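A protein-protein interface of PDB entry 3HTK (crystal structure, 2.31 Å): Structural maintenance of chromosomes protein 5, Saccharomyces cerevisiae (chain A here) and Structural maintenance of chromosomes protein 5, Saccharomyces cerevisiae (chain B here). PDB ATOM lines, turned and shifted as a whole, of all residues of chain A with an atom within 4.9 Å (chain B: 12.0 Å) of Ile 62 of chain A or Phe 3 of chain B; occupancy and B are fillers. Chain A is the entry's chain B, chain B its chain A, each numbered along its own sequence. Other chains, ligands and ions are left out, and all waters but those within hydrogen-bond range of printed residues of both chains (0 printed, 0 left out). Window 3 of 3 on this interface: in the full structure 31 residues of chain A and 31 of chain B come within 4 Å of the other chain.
The side-chain amino group (NZ) of Lys 7 of chain B lies within hydrogen-bond range of the side-chain amide oxygen (OD1) of Asn 59 of chain A (3.0 Å).
The side-chain hydroxyl of Thr 6 of chain B is in hydrogen-bond range of the backbone carbonyl oxygen of Phe 3 of chain B (2.8 Å). The side-chain carboxylate (OE1) of Glu 11 of chain B lies within salt-bridge range of the side-chain amino group (NZ) of Lys 7 of chain B, 3.98 Å away.
Among the printed residues, pairs that only touch across the chains: Met 58 of chain A with Thr 6 of chain B (3.9 Å), Met 58 of chain A with Lys 7 of chain B (3.6 Å), Met 58 of chain A with Leu 10 of chain B (3.3 Å), Ile 62 of chain A with Phe 3 of chain B (3.9 Å), Ile 62 of chain A with Lys 7 of chain B (3.5 Å) and Phe 65 of chain A with Phe 3 of chain B (3.8 Å).
Ile 62 of chain A touches two residues of chain B. Of the printed residues of chain A, Phe 3 of chain B touches Ile 62 and Phe 65. Met 58 of chain A touches just these residues of chain B: Thr 6 (3.9 Å), Lys 7 (3.6 Å) and Leu 10 (3.3 Å). Asn 59 of chain A touches just one residue of chain B: Lys 7 (3.0 Å). No residue of chain B comes within 4 Å of Asp 60 of chain A. No residue of chain B comes within 4 Å of Gly 63 of chain A. No residue of chain B comes within 4 Å of Phe 64 of chain A. Of the printed residues of chain A, Leu 10 of chain B touches Met 58 (3.3 Å). Printed residues of chain A within 4 Å of Thr 6 of chain B: Met 58. Of the printed residues of chain B, Phe 65 of chain A touches Phe 3. Printed residues of chain A within 4 Å of Lys 7 of chain B: Met 58, Asn 59 and Ile 62. Ala 4 of chain B touches none of the printed residues of chain A. Lys 1 of chain B touches none of the printed residues of chain A. The nearest residue of chain B that does not touch Ile 62 of chain A is Ala 4 of chain B (5.4 Å).
Printed residues of chain B that touch a printed residue of chain A: Phe 3, Thr 6, Lys 7 and Leu 10. Along chain B the printed residues that touch a printed residue of chain A span positions 3 to 10. Of the 9 printed residues of chain A, 4 touch a printed residue of chain B. Hydrophobic or aromatic side chains of chain A within 4 Å of the printed part of chain B: Met 58, Ile 62 and Phe 65. Along chain A the printed residues that touch a printed residue of chain B span positions 58 to 65. Among the printed residues, 7 pairs touch across the chains.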
ATOM      1  N   MET A  58      -6.344   7.566 -22.573  1.00  0.00           N
ATOM      2  CA  MET A  58      -6.713   6.599 -23.592  1.00  0.00           C
ATOM      3  C   MET A  58      -5.691   5.462 -23.519  1.00  0.00           C
ATOM      4  O   MET A  58      -6.055   4.291 -23.567  1.00  0.00           O
ATOM      5  CB  MET A  58      -6.648   7.257 -24.969  1.00  0.00           C
ATOM      6  CG  MET A  58      -7.293   6.463 -26.078  1.00  0.00           C
ATOM      7  SD  MET A  58      -9.039   6.863 -26.218  1.00  0.00           S
ATOM      8  CE  MET A  58      -9.063   7.814 -27.711  1.00  0.00           C
ATOM      9  N   ASN A  59      -4.408   5.813 -23.399  1.00  0.00           N
ATOM     10  CA  ASN A  59      -3.368   4.798 -23.309  1.00  0.00           C
ATOM     11  C   ASN A  59      -3.665   3.869 -22.139  1.00  0.00           C
ATOM     12  O   ASN A  59      -3.653   2.644 -22.298  1.00  0.00           O
ATOM     13  CB  ASN A  59      -1.978   5.429 -23.155  1.00  0.00           C
ATOM     14  CG  ASN A  59      -1.327   5.741 -24.501  1.00  0.00           C
ATOM     15  OD1 ASN A  59      -1.674   5.135 -25.517  1.00  0.00           O
ATOM     16  ND2 ASN A  59      -0.367   6.668 -24.510  1.00  0.00           N
ATOM     17  N   ASP A  60      -3.954   4.447 -20.974  1.00  0.00           N
ATOM     18  CA  ASP A  60      -4.277   3.648 -19.800  1.00  0.00           C
ATOM     19  C   ASP A  60      -5.401   2.663 -20.065  1.00  0.00           C
ATOM     20  O   ASP A  60      -5.209   1.455 -19.935  1.00  0.00           O
ATOM     21  CB  ASP A  60      -4.686   4.530 -18.626  1.00  0.00           C
ATOM     22  CG  ASP A  60      -3.517   4.957 -17.792  1.00  0.00           C
ATOM     23  OD1 ASP A  60      -3.738   5.556 -16.716  1.00  0.00           O
ATOM     24  OD2 ASP A  60      -2.379   4.688 -18.217  1.00  0.00           O
ATOM     25  N   VAL A  61      -6.572   3.176 -20.434  1.00  0.00           N
ATOM     26  CA  VAL A  61      -7.722   2.314 -20.690  1.00  0.00           C
ATOM     27  C   VAL A  61      -7.428   1.208 -21.691  1.00  0.00           C
ATOM     28  O   VAL A  61      -7.791   0.058 -21.466  1.00  0.00           O
ATOM     29  CB  VAL A  61      -8.934   3.124 -21.164  1.00  0.00           C
ATOM     30  CG1 VAL A  61     -10.058   2.202 -21.554  1.00  0.00           C
ATOM     31  CG2 VAL A  61      -9.395   4.036 -20.044  1.00  0.00           C
ATOM     32  N   ILE A  62      -6.785   1.558 -22.798  1.00  0.00           N
ATOM     33  CA  ILE A  62      -6.413   0.577 -23.814  1.00  0.00           C
ATOM     34  C   ILE A  62      -5.531  -0.485 -23.146  1.00  0.00           C
ATOM     35  O   ILE A  62      -5.699  -1.681 -23.381  1.00  0.00           O
ATOM     36  CB  ILE A  62      -5.614   1.245 -24.966  1.00  0.00           C
ATOM     37  CG1 ILE A  62      -6.556   2.072 -25.849  1.00  0.00           C
ATOM     38  CG2 ILE A  62      -4.871   0.184 -25.786  1.00  0.00           C
ATOM     39  CD1 ILE A  62      -5.825   2.946 -26.862  1.00  0.00           C
ATOM     40  N   GLY A  63      -4.585  -0.042 -22.322  1.00  0.00           N
ATOM     41  CA  GLY A  63      -3.713  -0.982 -21.638  1.00  0.00           C
ATOM     42  C   GLY A  63      -4.531  -1.960 -20.806  1.00  0.00           C
ATOM     43  O   GLY A  63      -4.260  -3.160 -20.790  1.00  0.00           O
ATOM     44  N   PHE A  64      -5.547  -1.453 -20.116  1.00  0.00           N
ATOM     45  CA  PHE A  64      -6.381  -2.311 -19.290  1.00  0.00           C
ATOM     46  C   PHE A  64      -7.232  -3.226 -20.154  1.00  0.00           C
ATOM     47  O   PHE A  64      -7.411  -4.400 -19.835  1.00  0.00           O
ATOM     48  CB  PHE A  64      -7.272  -1.473 -18.361  1.00  0.00           C
ATOM     49  CG  PHE A  64      -6.502  -0.657 -17.358  1.00  0.00           C
ATOM     50  CD1 PHE A  64      -5.345  -1.170 -16.763  1.00  0.00           C
ATOM     51  CD2 PHE A  64      -6.940   0.613 -16.991  1.00  0.00           C
ATOM     52  CE1 PHE A  64      -4.633  -0.426 -15.814  1.00  0.00           C
ATOM     53  CE2 PHE A  64      -6.245   1.365 -16.045  1.00  0.00           C
ATOM     54  CZ  PHE A  64      -5.088   0.849 -15.453  1.00  0.00           C
ATOM     55  N   PHE A  65      -7.752  -2.690 -21.250  1.00  0.00           N
ATOM     56  CA  PHE A  65      -8.570  -3.482 -22.154  1.00  0.00           C
ATOM     57  C   PHE A  65      -7.806  -4.719 -22.621  1.00  0.00           C
ATOM     58  O   PHE A  65      -8.325  -5.833 -22.552  1.00  0.00           O
ATOM     59  CB  PHE A  65      -8.970  -2.662 -23.377  1.00  0.00           C
ATOM     60  CG  PHE A  65      -9.942  -3.364 -24.282  1.00  0.00           C
ATOM     61  CD1 PHE A  65     -11.314  -3.197 -24.114  1.00  0.00           C
ATOM     62  CD2 PHE A  65      -9.486  -4.201 -25.296  1.00  0.00           C
ATOM     63  CE1 PHE A  65     -12.223  -3.856 -24.944  1.00  0.00           C
ATOM     64  CE2 PHE A  65     -10.381  -4.866 -26.133  1.00  0.00           C
ATOM     65  CZ  PHE A  65     -11.753  -4.692 -25.958  1.00  0.00           C
ATOM     66  N   ASN A  66      -6.575  -4.518 -23.092  1.00  0.00           N
ATOM     67  CA  ASN A  66      -5.749  -5.620 -23.585  1.00  0.00           C
ATOM     68  C   ASN A  66      -5.425  -6.677 -22.536  1.00  0.00           C
ATOM     69  O   ASN A  66      -4.959  -7.768 -22.873  1.00  0.00           O
ATOM     70  CB  ASN A  66      -4.436  -5.102 -24.182  1.00  0.00           C
ATOM     71  CG  ASN A  66      -4.640  -4.326 -25.464  1.00  0.00           C
ATOM     72  OD1 ASN A  66      -5.607  -4.548 -26.196  1.00  0.00           O
ATOM     73  ND2 ASN A  66      -3.712  -3.419 -25.757  1.00  0.00           N
ATOM     74  N   LYS B   1      -7.945  -3.503 -31.843  1.00  0.00           N
ATOM     75  CA  LYS B   1      -9.192  -3.458 -31.021  1.00  0.00           C
ATOM     76  C   LYS B   1     -10.075  -2.277 -31.407  1.00  0.00           C
ATOM     77  O   LYS B   1      -9.745  -1.514 -32.319  1.00  0.00           O
ATOM     78  CB  LYS B   1      -8.844  -3.385 -29.538  1.00  0.00           C
ATOM     79  N   PRO B   2     -11.190  -2.129 -30.698  1.00  0.00           N
ATOM     80  CA  PRO B   2     -12.157  -1.066 -30.971  1.00  0.00           C
ATOM     81  C   PRO B   2     -11.665   0.364 -30.735  1.00  0.00           C
ATOM     82  O   PRO B   2     -12.404   1.319 -30.967  1.00  0.00           O
ATOM     83  CB  PRO B   2     -13.433  -1.313 -30.160  1.00  0.00           C
ATOM     84  N   PHE B   3     -10.424   0.516 -30.286  1.00  0.00           N
ATOM     85  CA  PHE B   3      -9.885   1.844 -30.027  1.00  0.00           C
ATOM     86  C   PHE B   3      -8.908   2.333 -31.093  1.00  0.00           C
ATOM     87  O   PHE B   3      -8.925   3.504 -31.473  1.00  0.00           O
ATOM     88  CB  PHE B   3      -9.207   1.867 -28.656  1.00  0.00           C
ATOM     89  CG  PHE B   3     -10.144   1.580 -27.517  1.00  0.00           C
ATOM     90  CD1 PHE B   3     -10.400   0.273 -27.120  1.00  0.00           C
ATOM     91  CD2 PHE B   3     -10.804   2.620 -26.867  1.00  0.00           C
ATOM     92  CE1 PHE B   3     -11.306   0.005 -26.092  1.00  0.00           C
ATOM     93  CE2 PHE B   3     -11.708   2.364 -25.842  1.00  0.00           C
ATOM     94  CZ  PHE B   3     -11.961   1.055 -25.453  1.00  0.00           C
ATOM     95  N   ALA B   4      -8.067   1.420 -31.569  1.00  0.00           N
ATOM     96  CA  ALA B   4      -7.042   1.693 -32.577  1.00  0.00           C
ATOM     97  C   ALA B   4      -7.219   2.933 -33.464  1.00  0.00           C
ATOM     98  O   ALA B   4      -6.293   3.741 -33.589  1.00  0.00           O
ATOM     99  CB  ALA B   4      -6.860   0.457 -33.461  1.00  0.00           C
ATOM    100  N   ASN B   5      -8.394   3.080 -34.073  1.00  0.00           N
ATOM    101  CA  ASN B   5      -8.658   4.204 -34.971  1.00  0.00           C
ATOM    102  C   ASN B   5      -8.863   5.567 -34.316  1.00  0.00           C
ATOM    103  O   ASN B   5      -8.322   6.569 -34.789  1.00  0.00           O
ATOM    104  CB  ASN B   5      -9.845   3.877 -35.884  1.00  0.00           C
ATOM    105  CG  ASN B   5      -9.456   2.958 -37.036  1.00  0.00           C
ATOM    106  OD1 ASN B   5     -10.314   2.346 -37.674  1.00  0.00           O
ATOM    107  ND2 ASN B   5      -8.153   2.868 -37.313  1.00  0.00           N
ATOM    108  N   THR B   6      -9.647   5.616 -33.245  1.00  0.00           N
ATOM    109  CA  THR B   6      -9.875   6.883 -32.551  1.00  0.00           C
ATOM    110  C   THR B   6      -8.554   7.347 -31.956  1.00  0.00           C
ATOM    111  O   THR B   6      -8.138   8.490 -32.151  1.00  0.00           O
ATOM    112  CB  THR B   6     -10.882   6.738 -31.392  1.00  0.00           C
ATOM    113  OG1 THR B   6     -10.484   5.641 -30.566  1.00  0.00           O
ATOM    114  CG2 THR B   6     -12.297   6.511 -31.920  1.00  0.00           C
ATOM    115  N   LYS B   7      -7.898   6.443 -31.237  1.00  0.00           N
ATOM    116  CA  LYS B   7      -6.628   6.756 -30.600  1.00  0.00           C
ATOM    117  C   LYS B   7      -5.648   7.345 -31.608  1.00  0.00           C
ATOM    118  O   LYS B   7      -4.874   8.247 -31.285  1.00  0.00           O
ATOM    119  CB  LYS B   7      -6.034   5.497 -29.974  1.00  0.00           C
ATOM    120  CG  LYS B   7      -5.071   5.759 -28.813  1.00  0.00           C
ATOM    121  CD  LYS B   7      -3.736   6.309 -29.280  1.00  0.00           C
ATOM    122  CE  LYS B   7      -2.725   6.388 -28.135  1.00  0.00           C
ATOM    123  NZ  LYS B   7      -3.164   7.286 -27.049  1.00  0.00           N
ATOM    124  N   LYS B   8      -5.682   6.836 -32.833  1.00  0.00           N
ATOM    125  CA  LYS B   8      -4.783   7.339 -33.858  1.00  0.00           C
ATOM    126  C   LYS B   8      -5.140   8.799 -34.140  1.00  0.00           C
ATOM    127  O   LYS B   8      -4.268   9.656 -34.201  1.00  0.00           O
ATOM    128  CB  LYS B   8      -4.908   6.514 -35.146  1.00  0.00           C
ATOM    129  CG  LYS B   8      -3.670   6.570 -36.031  1.00  0.00           C
ATOM    130  CD  LYS B   8      -2.500   5.819 -35.381  1.00  0.00           C
ATOM    131  CE  LYS B   8      -1.219   5.919 -36.212  1.00  0.00           C
ATOM    132  NZ  LYS B   8      -0.109   5.096 -35.641  1.00  0.00           N
ATOM    133  N   THR B   9      -6.427   9.076 -34.308  1.00  0.00           N
ATOM    134  CA  THR B   9      -6.861  10.432 -34.579  1.00  0.00           C
ATOM    135  C   THR B   9      -6.501  11.340 -33.408  1.00  0.00           C
ATOM    136  O   THR B   9      -6.159  12.498 -33.609  1.00  0.00           O
ATOM    137  CB  THR B   9      -8.376  10.479 -34.861  1.00  0.00           C
ATOM    138  OG1 THR B   9      -8.654   9.723 -36.049  1.00  0.00           O
ATOM    139  CG2 THR B   9      -8.850  11.914 -35.079  1.00  0.00           C
ATOM    140  N   LEU B  10      -6.533  10.793 -32.195  1.00  0.00           N
ATOM    141  CA  LEU B  10      -6.200  11.546 -30.982  1.00  0.00           C
ATOM    142  C   LEU B  10      -4.716  11.907 -30.909  1.00  0.00           C
ATOM    143  O   LEU B  10      -4.355  13.027 -30.554  1.00  0.00           O
ATOM    144  CB  LEU B  10      -6.548  10.724 -29.737  1.00  0.00           C
ATOM    145  CG  LEU B  10      -7.338  11.324 -28.573  1.00  0.00           C
ATOM    146  CD1 LEU B  10      -7.085  10.441 -27.361  1.00  0.00           C
ATOM    147  CD2 LEU B  10      -6.921  12.761 -28.277  1.00  0.00           C
ATOM    148  N   GLU B  11      -3.862  10.936 -31.213  1.00  0.00           N
ATOM    149  CA  GLU B  11      -2.413  11.130 -31.185  1.00  0.00           C
ATOM    150  C   GLU B  11      -1.973  12.191 -32.185  1.00  0.00           C
ATOM    151  O   GLU B  11      -0.982  12.880 -31.966  1.00  0.00           O
ATOM    152  CB  GLU B  11      -1.687   9.832 -31.539  1.00  0.00           C
ATOM    153  CG  GLU B  11      -1.815   8.697 -30.544  1.00  0.00           C
ATOM    154  CD  GLU B  11      -1.088   7.434 -31.020  1.00  0.00           C
ATOM    155  OE1 GLU B  11      -0.850   6.521 -30.196  1.00  0.00           O
ATOM    156  OE2 GLU B  11      -0.761   7.354 -32.227  1.00  0.00           O
ATOM    157  N   ASN B  12      -2.700  12.303 -33.289  1.00  0.00           N
ATOM    158  CA  ASN B  12      -2.348  13.261 -34.313  1.00  0.00           C
ATOM    159  C   ASN B  12      -2.751  14.658 -33.916  1.00  0.00           C
ATOM    160  O   ASN B  12      -2.000  15.603 -34.142  1.00  0.00           O
ATOM    161  CB  ASN B  12      -2.988  12.887 -35.658  1.00  0.00           C
ATOM    162  CG  ASN B  12      -2.437  11.587 -36.222  1.00  0.00           C
ATOM    163  OD1 ASN B  12      -1.322  11.165 -35.873  1.00  0.00           O
ATOM    164  ND2 ASN B  12      -3.206  10.948 -37.108  1.00  0.00           N
ATOM    165  N   GLN B  13      -3.938  14.792 -33.330  1.00  0.00           N
ATOM    166  CA  GLN B  13      -4.422  16.093 -32.893  1.00  0.00           C
ATOM    167  C   GLN B  13      -3.445  16.653 -31.875  1.00  0.00           C
ATOM    168  O   GLN B  13      -3.113  17.832 -31.903  1.00  0.00           O
ATOM    169  CB  GLN B  13      -5.811  15.960 -32.276  1.00  0.00           C
ATOM    170  CG  GLN B  13      -6.761  15.197 -33.173  1.00  0.00           C
ATOM    171  CD  GLN B  13      -8.163  15.068 -32.609  1.00  0.00           C
ATOM    172  OE1 GLN B  13      -8.345  14.762 -31.426  1.00  0.00           O
ATOM    173  NE2 GLN B  13      -9.167  15.285 -33.463  1.00  0.00           N
